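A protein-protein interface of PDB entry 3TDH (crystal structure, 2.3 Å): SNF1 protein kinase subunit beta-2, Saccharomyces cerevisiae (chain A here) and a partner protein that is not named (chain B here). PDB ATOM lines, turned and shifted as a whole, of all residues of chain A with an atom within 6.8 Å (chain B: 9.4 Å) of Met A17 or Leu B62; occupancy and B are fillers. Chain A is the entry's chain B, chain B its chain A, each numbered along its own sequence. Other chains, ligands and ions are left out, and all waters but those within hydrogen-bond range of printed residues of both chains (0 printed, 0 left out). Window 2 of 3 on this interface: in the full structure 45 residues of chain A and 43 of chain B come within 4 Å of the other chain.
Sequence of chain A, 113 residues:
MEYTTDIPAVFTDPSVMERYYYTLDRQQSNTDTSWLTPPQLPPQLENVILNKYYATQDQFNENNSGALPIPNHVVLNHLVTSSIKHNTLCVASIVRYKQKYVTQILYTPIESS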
ATOM      1  N   ALA A   9      -0.942  37.637  -9.343  1.00  0.00           N
ATOM      2  CA  ALA A   9      -1.769  37.291 -10.503  1.00  0.00           C
ATOM      3  C   ALA A   9      -1.302  36.040 -11.249  1.00  0.00           C
ATOM      4  O   ALA A   9      -2.114  35.337 -11.853  1.00  0.00           O
ATOM      5  CB  ALA A   9      -1.861  38.479 -11.455  1.00  0.00           C
ATOM      6  N   VAL A  10       0.000  35.765 -11.189  1.00  0.00           N
ATOM      7  CA  VAL A  10       0.597  34.598 -11.848  1.00  0.00           C
ATOM      8  C   VAL A  10       0.054  33.250 -11.331  1.00  0.00           C
ATOM      9  O   VAL A  10       0.173  32.228 -12.012  1.00  0.00           O
ATOM     10  CB  VAL A  10       2.163  34.654 -11.800  1.00  0.00           C
ATOM     11  CG1 VAL A  10       2.693  34.441 -10.383  1.00  0.00           C
ATOM     12  CG2 VAL A  10       2.788  33.657 -12.777  1.00  0.00           C
ATOM     13  N   PHE A  11      -0.554  33.253 -10.146  1.00  0.00           N
ATOM     14  CA  PHE A  11      -1.098  32.019  -9.570  1.00  0.00           C
ATOM     15  C   PHE A  11      -2.629  31.940  -9.576  1.00  0.00           C
ATOM     16  O   PHE A  11      -3.203  30.929  -9.168  1.00  0.00           O
ATOM     17  CB  PHE A  11      -0.544  31.782  -8.153  1.00  0.00           C
ATOM     18  CG  PHE A  11       0.957  31.838  -8.069  1.00  0.00           C
ATOM     19  CD1 PHE A  11       1.746  30.969  -8.822  1.00  0.00           C
ATOM     20  CD2 PHE A  11       1.584  32.759  -7.235  1.00  0.00           C
ATOM     21  CE1 PHE A  11       3.139  31.026  -8.755  1.00  0.00           C
ATOM     22  CE2 PHE A  11       2.974  32.821  -7.156  1.00  0.00           C
ATOM     23  CZ  PHE A  11       3.755  31.951  -7.917  1.00  0.00           C
ATOM     24  N   ASP A  13      -4.363  33.764 -12.453  1.00  0.00           N
ATOM     25  CA  ASP A  13      -4.725  34.137 -13.822  1.00  0.00           C
ATOM     26  C   ASP A  13      -3.776  33.495 -14.841  1.00  0.00           C
ATOM     27  O   ASP A  13      -2.590  33.830 -14.880  1.00  0.00           O
ATOM     28  CB  ASP A  13      -4.724  35.664 -13.969  1.00  0.00           C
ATOM     29  CG  ASP A  13      -5.245  36.140 -15.324  1.00  0.00           C
ATOM     30  OD1 ASP A  13      -5.614  35.308 -16.184  1.00  0.00           O
ATOM     31  OD2 ASP A  13      -5.284  37.371 -15.524  1.00  0.00           O
ATOM     32  N   PRO A  14      -4.302  32.577 -15.676  1.00  0.00           N
ATOM     33  CA  PRO A  14      -3.509  31.889 -16.701  1.00  0.00           C
ATOM     34  C   PRO A  14      -2.808  32.827 -17.688  1.00  0.00           C
ATOM     35  O   PRO A  14      -1.780  32.453 -18.253  1.00  0.00           O
ATOM     36  CB  PRO A  14      -4.551  31.040 -17.436  1.00  0.00           C
ATOM     37  CG  PRO A  14      -5.619  30.812 -16.433  1.00  0.00           C
ATOM     38  CD  PRO A  14      -5.695  32.090 -15.653  1.00  0.00           C
ATOM     39  N   SER A  15      -3.356  34.028 -17.879  1.00  0.00           N
ATOM     40  CA  SER A  15      -2.800  35.016 -18.811  1.00  0.00           C
ATOM     41  C   SER A  15      -1.363  35.417 -18.484  1.00  0.00           C
ATOM     42  O   SER A  15      -0.554  35.629 -19.387  1.00  0.00           O
ATOM     43  CB  SER A  15      -3.676  36.274 -18.847  1.00  0.00           C
ATOM     44  OG  SER A  15      -5.014  35.969 -19.195  1.00  0.00           O
ATOM     45  N   VAL A  16      -1.057  35.516 -17.191  1.00  0.00           N
ATOM     46  CA  VAL A  16       0.236  36.024 -16.719  1.00  0.00           C
ATOM     47  C   VAL A  16       1.397  35.090 -17.078  1.00  0.00           C
ATOM     48  O   VAL A  16       2.377  35.525 -17.691  1.00  0.00           O
ATOM     49  CB  VAL A  16       0.210  36.331 -15.195  1.00  0.00           C
ATOM     50  CG1 VAL A  16       1.524  36.956 -14.741  1.00  0.00           C
ATOM     51  CG2 VAL A  16      -0.952  37.262 -14.862  1.00  0.00           C
ATOM     52  N   MET A  17       1.280  33.815 -16.707  1.00  0.00           N
ATOM     53  CA  MET A  17       2.300  32.816 -17.034  1.00  0.00           C
ATOM     54  C   MET A  17       2.404  32.583 -18.542  1.00  0.00           C
ATOM     55  O   MET A  17       3.501  32.373 -19.069  1.00  0.00           O
ATOM     56  CB  MET A  17       2.034  31.494 -16.302  1.00  0.00           C
ATOM     57  CG  MET A  17       3.171  30.472 -16.393  1.00  0.00           C
ATOM     58  SD  MET A  17       4.757  31.109 -15.799  1.00  0.00           S
ATOM     59  CE  MET A  17       5.768  29.632 -15.854  1.00  0.00           C
ATOM     60  N   GLU A  18       1.258  32.623 -19.225  1.00  0.00           N
ATOM     61  CA  GLU A  18       1.208  32.513 -20.685  1.00  0.00           C
ATOM     62  C   GLU A  18       2.035  33.619 -21.340  1.00  0.00           C
ATOM     63  O   GLU A  18       2.841  33.349 -22.233  1.00  0.00           O
ATOM     64  CB  GLU A  18      -0.240  32.554 -21.188  1.00  0.00           C
ATOM     65  CG  GLU A  18      -0.383  32.395 -22.701  1.00  0.00           C
ATOM     66  CD  GLU A  18      -1.819  32.539 -23.186  1.00  0.00           C
ATOM     67  OE1 GLU A  18      -2.477  33.547 -22.842  1.00  0.00           O
ATOM     68  OE2 GLU A  18      -2.281  31.647 -23.927  1.00  0.00           O
ATOM     69  N   ARG A  19       1.837  34.852 -20.878  1.00  0.00           N
ATOM     70  CA  ARG A  19       2.597  36.009 -21.353  1.00  0.00           C
ATOM     71  C   ARG A  19       4.107  35.794 -21.207  1.00  0.00           C
ATOM     72  O   ARG A  19       4.872  36.160 -22.103  1.00  0.00           O
ATOM     73  CB  ARG A  19       2.165  37.277 -20.606  1.00  0.00           C
ATOM     74  CG  ARG A  19       2.604  38.589 -21.253  1.00  0.00           C
ATOM     75  CD  ARG A  19       1.574  39.081 -22.256  1.00  0.00           C
ATOM     76  NE  ARG A  19       2.053  40.220 -23.042  1.00  0.00           N
ATOM     77  CZ  ARG A  19       1.360  40.808 -24.014  1.00  0.00           C
ATOM     78  NH1 ARG A  19       0.148  40.371 -24.336  1.00  0.00           N
ATOM     79  NH2 ARG A  19       1.881  41.838 -24.669  1.00  0.00           N
ATOM     80  N   TYR A  20       4.527  35.196 -20.088  1.00  0.00           N
ATOM     81  CA  TYR A  20       5.939  34.879 -19.856  1.00  0.00           C
ATOM     82  C   TYR A  20       6.476  33.866 -20.867  1.00  0.00           C
ATOM     83  O   TYR A  20       7.574  34.043 -21.395  1.00  0.00           O
ATOM     84  CB  TYR A  20       6.181  34.364 -18.428  1.00  0.00           C
ATOM     85  CG  TYR A  20       5.907  35.357 -17.315  1.00  0.00           C
ATOM     86  CD1 TYR A  20       6.298  36.694 -17.422  1.00  0.00           C
ATOM     87  CD2 TYR A  20       5.284  34.946 -16.139  1.00  0.00           C
ATOM     88  CE1 TYR A  20       6.050  37.602 -16.392  1.00  0.00           C
ATOM     89  CE2 TYR A  20       5.035  35.841 -15.101  1.00  0.00           C
ATOM     90  CZ  TYR A  20       5.419  37.166 -15.233  1.00  0.00           C
ATOM     91  OH  TYR A  20       5.171  38.049 -14.206  1.00  0.00           O
ATOM     92  N   TYR A  21       5.702  32.811 -21.127  1.00  0.00           N
ATOM     93  CA  TYR A  21       6.083  31.790 -22.107  1.00  0.00           C
ATOM     94  C   TYR A  21       6.306  32.382 -23.501  1.00  0.00           C
ATOM     95  O   TYR A  21       7.312  32.089 -24.152  1.00  0.00           O
ATOM     96  CB  TYR A  21       5.026  30.681 -22.200  1.00  0.00           C
ATOM     97  CG  TYR A  21       4.958  29.724 -21.026  1.00  0.00           C
ATOM     98  CD1 TYR A  21       6.117  29.232 -20.418  1.00  0.00           C
ATOM     99  CD2 TYR A  21       3.727  29.277 -20.547  1.00  0.00           C
ATOM    100  CE1 TYR A  21       6.046  28.343 -19.345  1.00  0.00           C
ATOM    101  CE2 TYR A  21       3.645  28.386 -19.479  1.00  0.00           C
ATOM    102  CZ  TYR A  21       4.807  27.923 -18.884  1.00  0.00           C
ATOM    103  OH  TYR A  21       4.726  27.044 -17.829  1.00  0.00           O
ATOM    104  N   TYR A  22       5.369  33.220 -23.943  1.00  0.00           N
ATOM    105  CA  TYR A  22       5.370  33.734 -25.314  1.00  0.00           C
ATOM    106  C   TYR A  22       6.360  34.872 -25.566  1.00  0.00           C
ATOM    107  O   TYR A  22       6.893  34.994 -26.671  1.00  0.00           O
ATOM    108  CB  TYR A  22       3.957  34.135 -25.748  1.00  0.00           C
ATOM    109  CG  TYR A  22       3.108  32.972 -26.222  1.00  0.00           C
ATOM    110  CD1 TYR A  22       3.176  32.524 -27.544  1.00  0.00           C
ATOM    111  CD2 TYR A  22       2.235  32.321 -25.352  1.00  0.00           C
ATOM    112  CE1 TYR A  22       2.398  31.452 -27.982  1.00  0.00           C
ATOM    113  CE2 TYR A  22       1.454  31.253 -25.780  1.00  0.00           C
ATOM    114  CZ  TYR A  22       1.541  30.823 -27.094  1.00  0.00           C
ATOM    115  OH  TYR A  22       0.768  29.767 -27.516  1.00  0.00           O
ATOM    116  N   TRP A  35      14.199  30.858 -14.545  1.00  0.00           N
ATOM    117  CA  TRP A  35      13.248  31.544 -13.660  1.00  0.00           C
ATOM    118  C   TRP A  35      11.790  31.088 -13.815  1.00  0.00           C
ATOM    119  O   TRP A  35      10.952  31.381 -12.961  1.00  0.00           O
ATOM    120  CB  TRP A  35      13.374  33.072 -13.785  1.00  0.00           C
ATOM    121  CG  TRP A  35      12.847  33.676 -15.072  1.00  0.00           C
ATOM    122  CD1 TRP A  35      11.535  33.884 -15.406  1.00  0.00           C
ATOM    123  CD2 TRP A  35      13.624  34.181 -16.170  1.00  0.00           C
ATOM    124  NE1 TRP A  35      11.450  34.468 -16.649  1.00  0.00           N
ATOM    125  CE2 TRP A  35      12.714  34.663 -17.139  1.00  0.00           C
ATOM    126  CE3 TRP A  35      15.000  34.264 -16.432  1.00  0.00           C
ATOM    127  CZ2 TRP A  35      13.136  35.223 -18.355  1.00  0.00           C
ATOM    128  CZ3 TRP A  35      15.421  34.823 -17.643  1.00  0.00           C
ATOM    129  CH2 TRP A  35      14.488  35.293 -18.588  1.00  0.00           C
ATOM    130  N   LEU A  36      11.503  30.367 -14.897  1.00  0.00           N
ATOM    131  CA  LEU A  36      10.161  29.846 -15.165  1.00  0.00           C
ATOM    132  C   LEU A  36       9.891  28.549 -14.402  1.00  0.00           C
ATOM    133  O   LEU A  36       8.767  28.045 -14.383  1.00  0.00           O
ATOM    134  CB  LEU A  36       9.966  29.620 -16.670  1.00  0.00           C
ATOM    135  CG  LEU A  36      10.044  30.831 -17.608  1.00  0.00           C
ATOM    136  CD1 LEU A  36      10.363  30.386 -19.028  1.00  0.00           C
ATOM    137  CD2 LEU A  36       8.763  31.656 -17.569  1.00  0.00           C
ATOM    138  N   THR A  37      10.939  28.018 -13.778  1.00  0.00           N
ATOM    139  CA  THR A  37      10.873  26.773 -13.023  1.00  0.00           C
ATOM    140  C   THR A  37      11.526  26.975 -11.650  1.00  0.00           C
ATOM    141  O   THR A  37      12.537  27.674 -11.545  1.00  0.00           O
ATOM    142  CB  THR A  37      11.553  25.623 -13.811  1.00  0.00           C
ATOM    143  OG1 THR A  37      10.747  25.291 -14.947  1.00  0.00           O
ATOM    144  CG2 THR A  37      11.732  24.373 -12.962  1.00  0.00           C
ATOM    145  N   PRO A  38      10.932  26.392 -10.588  1.00  0.00           N
ATOM    146  CA  PRO A  38      11.555  26.428  -9.263  1.00  0.00           C
ATOM    147  C   PRO A  38      12.948  25.795  -9.266  1.00  0.00           C
ATOM    148  O   PRO A  38      13.173  24.820  -9.987  1.00  0.00           O
ATOM    149  CB  PRO A  38      10.593  25.607  -8.392  1.00  0.00           C
ATOM    150  CG  PRO A  38       9.704  24.877  -9.352  1.00  0.00           C
ATOM    151  CD  PRO A  38       9.602  25.759 -10.544  1.00  0.00           C
ATOM    152  N   SER B  57       5.298  17.842  -2.021  1.00  0.00           N
ATOM    153  CA  SER B  57       4.047  17.898  -2.771  1.00  0.00           C
ATOM    154  C   SER B  57       4.206  17.197  -4.113  1.00  0.00           C
ATOM    155  O   SER B  57       5.242  17.320  -4.769  1.00  0.00           O
ATOM    156  CB  SER B  57       3.604  19.347  -2.981  1.00  0.00           C
ATOM    157  OG  SER B  57       2.322  19.407  -3.583  1.00  0.00           O
ATOM    158  N   SER B  59       1.953  17.652  -6.627  1.00  0.00           N
ATOM    159  CA  SER B  59       1.379  18.553  -7.632  1.00  0.00           C
ATOM    160  C   SER B  59       2.465  19.303  -8.410  1.00  0.00           C
ATOM    161  O   SER B  59       3.655  19.002  -8.280  1.00  0.00           O
ATOM    162  CB  SER B  59       0.423  19.545  -6.963  1.00  0.00           C
ATOM    163  OG  SER B  59      -0.523  18.873  -6.147  1.00  0.00           O
ATOM    164  N   TYR B  60       2.058  20.283  -9.213  1.00  0.00           N
ATOM    165  CA  TYR B  60       2.995  21.039 -10.046  1.00  0.00           C
ATOM    166  C   TYR B  60       3.147  22.492  -9.567  1.00  0.00           C
ATOM    167  O   TYR B  60       2.267  22.993  -8.863  1.00  0.00           O
ATOM    168  CB  TYR B  60       2.593  20.927 -11.524  1.00  0.00           C
ATOM    169  CG  TYR B  60       2.606  19.496 -12.024  1.00  0.00           C
ATOM    170  CD1 TYR B  60       3.808  18.857 -12.341  1.00  0.00           C
ATOM    171  CD2 TYR B  60       1.420  18.772 -12.162  1.00  0.00           C
ATOM    172  CE1 TYR B  60       3.827  17.534 -12.787  1.00  0.00           C
ATOM    173  CE2 TYR B  60       1.430  17.451 -12.612  1.00  0.00           C
ATOM    174  CZ  TYR B  60       2.635  16.840 -12.922  1.00  0.00           C
ATOM    175  OH  TYR B  60       2.651  15.537 -13.367  1.00  0.00           O
ATOM    176  N   PRO B  61       4.265  23.162  -9.930  1.00  0.00           N
ATOM    177  CA  PRO B  61       4.691  24.448  -9.351  1.00  0.00           C
ATOM    178  C   PRO B  61       3.601  25.495  -9.108  1.00  0.00           C
ATOM    179  O   PRO B  61       3.423  25.938  -7.969  1.00  0.00           O
ATOM    180  CB  PRO B  61       5.715  24.962 -10.366  1.00  0.00           C
ATOM    181  CG  PRO B  61       6.320  23.739 -10.916  1.00  0.00           C
ATOM    182  CD  PRO B  61       5.223  22.701 -10.955  1.00  0.00           C
ATOM    183  N   LEU B  62       2.887  25.890 -10.165  1.00  0.00           N
ATOM    184  CA  LEU B  62       1.859  26.932 -10.067  1.00  0.00           C
ATOM    185  C   LEU B  62       0.697  26.502  -9.174  1.00  0.00           C
ATOM    186  O   LEU B  62       0.134  27.319  -8.442  1.00  0.00           O
ATOM    187  CB  LEU B  62       1.339  27.331 -11.455  1.00  0.00           C
ATOM    188  CG  LEU B  62       2.298  28.011 -12.440  1.00  0.00           C
ATOM    189  CD1 LEU B  62       1.785  27.864 -13.871  1.00  0.00           C
ATOM    190  CD2 LEU B  62       2.518  29.481 -12.088  1.00  0.00           C
ATOM    191  N   ASP B  63       0.352  25.218  -9.246  1.00  0.00           N
ATOM    192  CA  ASP B  63      -0.693  24.637  -8.406  1.00  0.00           C
ATOM    193  C   ASP B  63      -0.303  24.680  -6.927  1.00  0.00           C
ATOM    194  O   ASP B  63      -1.109  25.079  -6.083  1.00  0.00           O
ATOM    195  CB  ASP B  63      -0.993  23.198  -8.848  1.00  0.00           C
ATOM    196  CG  ASP B  63      -2.225  22.619  -8.175  1.00  0.00           C
ATOM    197  OD1 ASP B  63      -3.233  23.343  -8.020  1.00  0.00           O
ATOM    198  OD2 ASP B  63      -2.189  21.425  -7.809  1.00  0.00           O
ATOM    199  N   VAL B  64       0.937  24.284  -6.627  1.00  0.00           N
ATOM    200  CA  VAL B  64       1.455  24.285  -5.253  1.00  0.00           C
ATOM    201  C   VAL B  64       1.485  25.704  -4.684  1.00  0.00           C
ATOM    202  O   VAL B  64       0.932  25.960  -3.610  1.00  0.00           O
ATOM    203  CB  VAL B  64       2.870  23.640  -5.160  1.00  0.00           C
ATOM    204  CG1 VAL B  64       3.435  23.749  -3.742  1.00  0.00           C
ATOM    205  CG2 VAL B  64       2.830  22.182  -5.605  1.00  0.00           C
ATOM    206  N   MET B  65       2.113  26.621  -5.417  1.00  0.00           N
ATOM    207  CA  MET B  65       2.198  28.024  -5.002  1.00  0.00           C
ATOM    208  C   MET B  65       0.818  28.618  -4.728  1.00  0.00           C
ATOM    209  O   MET B  65       0.653  29.412  -3.799  1.00  0.00           O
ATOM    210  CB  MET B  65       2.934  28.864  -6.049  1.00  0.00           C
ATOM    211  CG  MET B  65       4.404  28.494  -6.264  1.00  0.00           C
ATOM    212  SD  MET B  65       5.460  28.626  -4.799  1.00  0.00           S
ATOM    213  CE  MET B  65       5.450  30.397  -4.524  1.00  0.00           C
ATOM    214  N   GLY B  66      -0.163  28.219  -5.537  1.00  0.00           N
ATOM    215  CA  GLY B  66      -1.550  28.651  -5.369  1.00  0.00           C
ATOM    216  C   GLY B  66      -2.172  28.165  -4.072  1.00  0.00           C
ATOM    217  O   GLY B  66      -2.848  28.926  -3.388  1.00  0.00           O
ATOM    218  N   GLU B  67      -1.940  26.898  -3.739  1.00  0.00           N
ATOM    219  CA  GLU B  67      -2.420  26.322  -2.479  1.00  0.00           C
ATOM    220  C   GLU B  67      -1.832  27.030  -1.256  1.00  0.00           C
ATOM    221  O   GLU B  67      -2.535  27.264  -0.272  1.00  0.00           O
ATOM    222  CB  GLU B  67      -2.102  24.827  -2.406  1.00  0.00           C
ATOM    223  CG  GLU B  67      -2.883  23.964  -3.389  1.00  0.00           C
ATOM    224  CD  GLU B  67      -2.616  22.479  -3.207  1.00  0.00           C
ATOM    225  OE1 GLU B  67      -3.588  21.693  -3.259  1.00  0.00           O
ATOM    226  OE2 GLU B  67      -1.441  22.093  -3.006  1.00  0.00           O
ATOM    227  N   ILE B  68      -0.548  27.374  -1.333  1.00  0.00           N
ATOM    228  CA  ILE B  68       0.153  28.032  -0.231  1.00  0.00           C
ATOM    229  C   ILE B  68      -0.412  29.430   0.024  1.00  0.00           C
ATOM    230  O   ILE B  68      -0.785  29.756   1.155  1.00  0.00           O
ATOM    231  CB  ILE B  68       1.688  28.091  -0.469  1.00  0.00           C
ATOM    232  CG1 ILE B  68       2.265  26.677  -0.601  1.00  0.00           C
ATOM    233  CG2 ILE B  68       2.382  28.844   0.662  1.00  0.00           C
ATOM    234  CD1 ILE B  68       3.684  26.625  -1.137  1.00  0.00           C
ATOM    235  N   TYR B  69      -0.485  30.242  -1.033  1.00  0.00           N
ATOM    236  CA  TYR B  69      -1.041  31.594  -0.945  1.00  0.00           C
ATOM    237  C   TYR B  69      -2.473  31.614  -0.404  1.00  0.00           C
ATOM    238  O   TYR B  69      -2.809  32.466   0.419  1.00  0.00           O
ATOM    239  CB  TYR B  69      -0.956  32.316  -2.296  1.00  0.00           C
ATOM    240  CG  TYR B  69       0.365  33.016  -2.537  1.00  0.00           C
ATOM    241  CD1 TYR B  69       0.674  34.210  -1.883  1.00  0.00           C
ATOM    242  CD2 TYR B  69       1.305  32.488  -3.422  1.00  0.00           C
ATOM    243  CE1 TYR B  69       1.885  34.855  -2.097  1.00  0.00           C
ATOM    244  CE2 TYR B  69       2.518  33.126  -3.647  1.00  0.00           C
ATOM    245  CZ  TYR B  69       2.801  34.308  -2.982  1.00  0.00           C
ATOM    246  OH  TYR B  69       4.002  34.943  -3.202  1.00  0.00           O
ATOM    247  N   ILE B  70      -3.303  30.677  -0.863  1.00  0.00           N
ATOM    248  CA  ILE B  70      -4.670  30.515  -0.346  1.00  0.00           C
ATOM    249  C   ILE B  70      -4.660  30.236   1.165  1.00  0.00           C
ATOM    250  O   ILE B  70      -5.392  30.877   1.924  1.00  0.00           O
ATOM    251  CB  ILE B  70      -5.463  29.416  -1.120  1.00  0.00           C
ATOM    252  CG1 ILE B  70      -5.753  29.878  -2.556  1.00  0.00           C
ATOM    253  CG2 ILE B  70      -6.781  29.076  -0.411  1.00  0.00           C
ATOM    254  CD1 ILE B  70      -6.186  28.765  -3.520  1.00  0.00           C
ATOM    255  N   GLU B  84       9.924  38.617 -11.332  1.00  0.00           N
ATOM    256  CA  GLU B  84      10.110  37.522 -12.286  1.00  0.00           C
ATOM    257  C   GLU B  84      11.309  36.622 -11.977  1.00  0.00           C
ATOM    258  O   GLU B  84      11.348  35.470 -12.413  1.00  0.00           O
ATOM    259  CB  GLU B  84      10.221  38.074 -13.711  1.00  0.00           C
ATOM    260  N   LEU B  87       9.813  34.174  -8.552  1.00  0.00           N
ATOM    261  CA  LEU B  87       8.401  33.780  -8.590  1.00  0.00           C
ATOM    262  C   LEU B  87       8.048  32.728  -7.539  1.00  0.00           C
ATOM    263  O   LEU B  87       6.930  32.705  -7.025  1.00  0.00           O
ATOM    264  CB  LEU B  87       8.030  33.244  -9.980  1.00  0.00           C
ATOM    265  CG  LEU B  87       7.995  34.175 -11.201  1.00  0.00           C
ATOM    266  CD1 LEU B  87       7.860  33.353 -12.473  1.00  0.00           C
ATOM    267  CD2 LEU B  87       6.873  35.201 -11.106  1.00  0.00           C
ATOM    268  N   TRP B  88       9.013  31.868  -7.223  1.00  0.00           N
ATOM    269  CA  TRP B  88       8.781  30.715  -6.359  1.00  0.00           C
ATOM    270  C   TRP B  88       9.212  30.977  -4.911  1.00  0.00           C
ATOM    271  O   TRP B  88       9.425  30.044  -4.132  1.00  0.00           O
ATOM    272  CB  TRP B  88       9.482  29.488  -6.950  1.00  0.00           C
ATOM    273  CG  TRP B  88       9.370  29.452  -8.449  1.00  0.00           C
ATOM    274  CD1 TRP B  88      10.352  29.741  -9.350  1.00  0.00           C
ATOM    275  CD2 TRP B  88       8.195  29.154  -9.215  1.00  0.00           C
ATOM    276  NE1 TRP B  88       9.869  29.623 -10.630  1.00  0.00           N
ATOM    277  CE2 TRP B  88       8.548  29.264 -10.577  1.00  0.00           C
ATOM    278  CE3 TRP B  88       6.882  28.796  -8.883  1.00  0.00           C
ATOM    279  CZ2 TRP B  88       7.634  29.026 -11.611  1.00  0.00           C
ATOM    280  CZ3 TRP B  88       5.971  28.563  -9.912  1.00  0.00           C
ATOM    281  CH2 TRP B  88       6.355  28.677 -11.260  1.00  0.00           C
ATOM    282  N   LEU B 118      10.014  27.304  -2.921  1.00  0.00           N
ATOM    283  CA  LEU B 118       9.671  26.063  -3.601  1.00  0.00           C
ATOM    284  C   LEU B 118      10.896  25.497  -4.312  1.00  0.00           C
ATOM    285  O   LEU B 118      11.583  26.205  -5.053  1.00  0.00           O
ATOM    286  CB  LEU B 118       8.519  26.283  -4.595  1.00  0.00           C
ATOM    287  CG  LEU B 118       7.874  25.054  -5.249  1.00  0.00           C
ATOM    288  CD1 LEU B 118       7.189  24.160  -4.218  1.00  0.00           C
ATOM    289  CD2 LEU B 118       6.882  25.471  -6.341  1.00  0.00           C
ATOM    290  N   TYR B 126       8.007  18.006  -5.515  1.00  0.00           N
ATOM    291  CA  TYR B 126       8.468  19.324  -5.085  1.00  0.00           C
ATOM    292  C   TYR B 126       8.489  19.457  -3.563  1.00  0.00           C
ATOM    293  O   TYR B 126       7.652  18.878  -2.867  1.00  0.00           O
ATOM    294  CB  TYR B 126       7.603  20.427  -5.708  1.00  0.00           C
ATOM    295  CG  TYR B 126       7.697  20.489  -7.215  1.00  0.00           C
ATOM    296  CD1 TYR B 126       8.638  21.302  -7.839  1.00  0.00           C
ATOM    297  CD2 TYR B 126       6.849  19.725  -8.019  1.00  0.00           C
ATOM    298  CE1 TYR B 126       8.731  21.359  -9.227  1.00  0.00           C
ATOM    299  CE2 TYR B 126       6.936  19.773  -9.408  1.00  0.00           C
ATOM    300  CZ  TYR B 126       7.877  20.591 -10.004  1.00  0.00           C
ATOM    301  OH  TYR B 126       7.969  20.644 -11.376  1.00  0.00           O
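The backbone carbonyl oxygen of Trp A35 sits at hydrogen-bond distance from the indole nitrogen of Trp B88 (3.1 Å).
The backbone carbonyl oxygen (O) of Thr A37 sits close to the indole nitrogen (NE1) of Trp B88 (3.4 Å).
N of Pro A38 sits close to NE1 of Trp B88, 3.4 Å away.
The backbone NH (N) of Leu B118 sits at hydrogen-bond distance from the backbone carbonyl oxygen (O) of Trp B88.
The backbone carbonyl oxygen of Tyr B126 is in hydrogen-bond range of the backbone NH of Ser B57 (2.7 Å).
Among the printed residues, merely in contact across the chains: Val A10 with Leu B62 (3.6 Å), Phe A11 with Leu B62 (3.7 Å), Phe A11 with Met B65 (3.5 Å), Phe A11 with Tyr B69 (3.6 Å), Phe A11 with Leu B87 (3.4 Å), Phe A11 with Trp B88 (3.9 Å), Met A17 with Leu B62 (3.9 Å), Trp A35 with Glu B84 (3.4 Å), Trp A35 with Leu B87 (3.7 Å), Leu A36 with Trp B88 (3.2 Å), Pro A38 with Pro B61 (3.9 Å), Pro A38 with Leu B118 (3.5 Å) and Pro A38 with Tyr B126 (3.7 Å).
Pro A14 touches none of the printed residues of chain B.
No residue of chain B comes within 4 Å of Val A16.
Met A17 touches one residue of chain B.
Tyr A21 touches none of the printed residues of chain B.
Of the printed residues of chain B, Thr A37 touches Trp B88.
Printed residues of chain B within 4 Å of Pro A38: Pro B61 (3.9 Å), Trp B88 (3.4 Å), Leu B118 (3.5 Å) and Tyr B126 (3.7 Å).
The nearest residue of chain A that does not touch Leu B62 is Tyr A21 (5.0 Å).
The nearest printed residue of chain A that does not touch Glu B84 is Tyr A20 (5.0 Å).
Of the 18 printed residues of chain B, 9 touch a printed residue of chain A.
Hydrophobic or aromatic side chains of chain B that line the printed part of chain A: Pro B61, Leu B62, Met B65, Tyr B69, Leu B87, Trp B88 and Tyr B126.
Of the 17 printed residues of chain A, 7 touch a printed residue of chain B.
Hydrophobic or aromatic side chains of chain A within 4 Å of the printed part of chain B: Phe A11, Met A17, Trp A35 and Pro A38.
Among the printed residues, 16 pairs touch across the chains.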
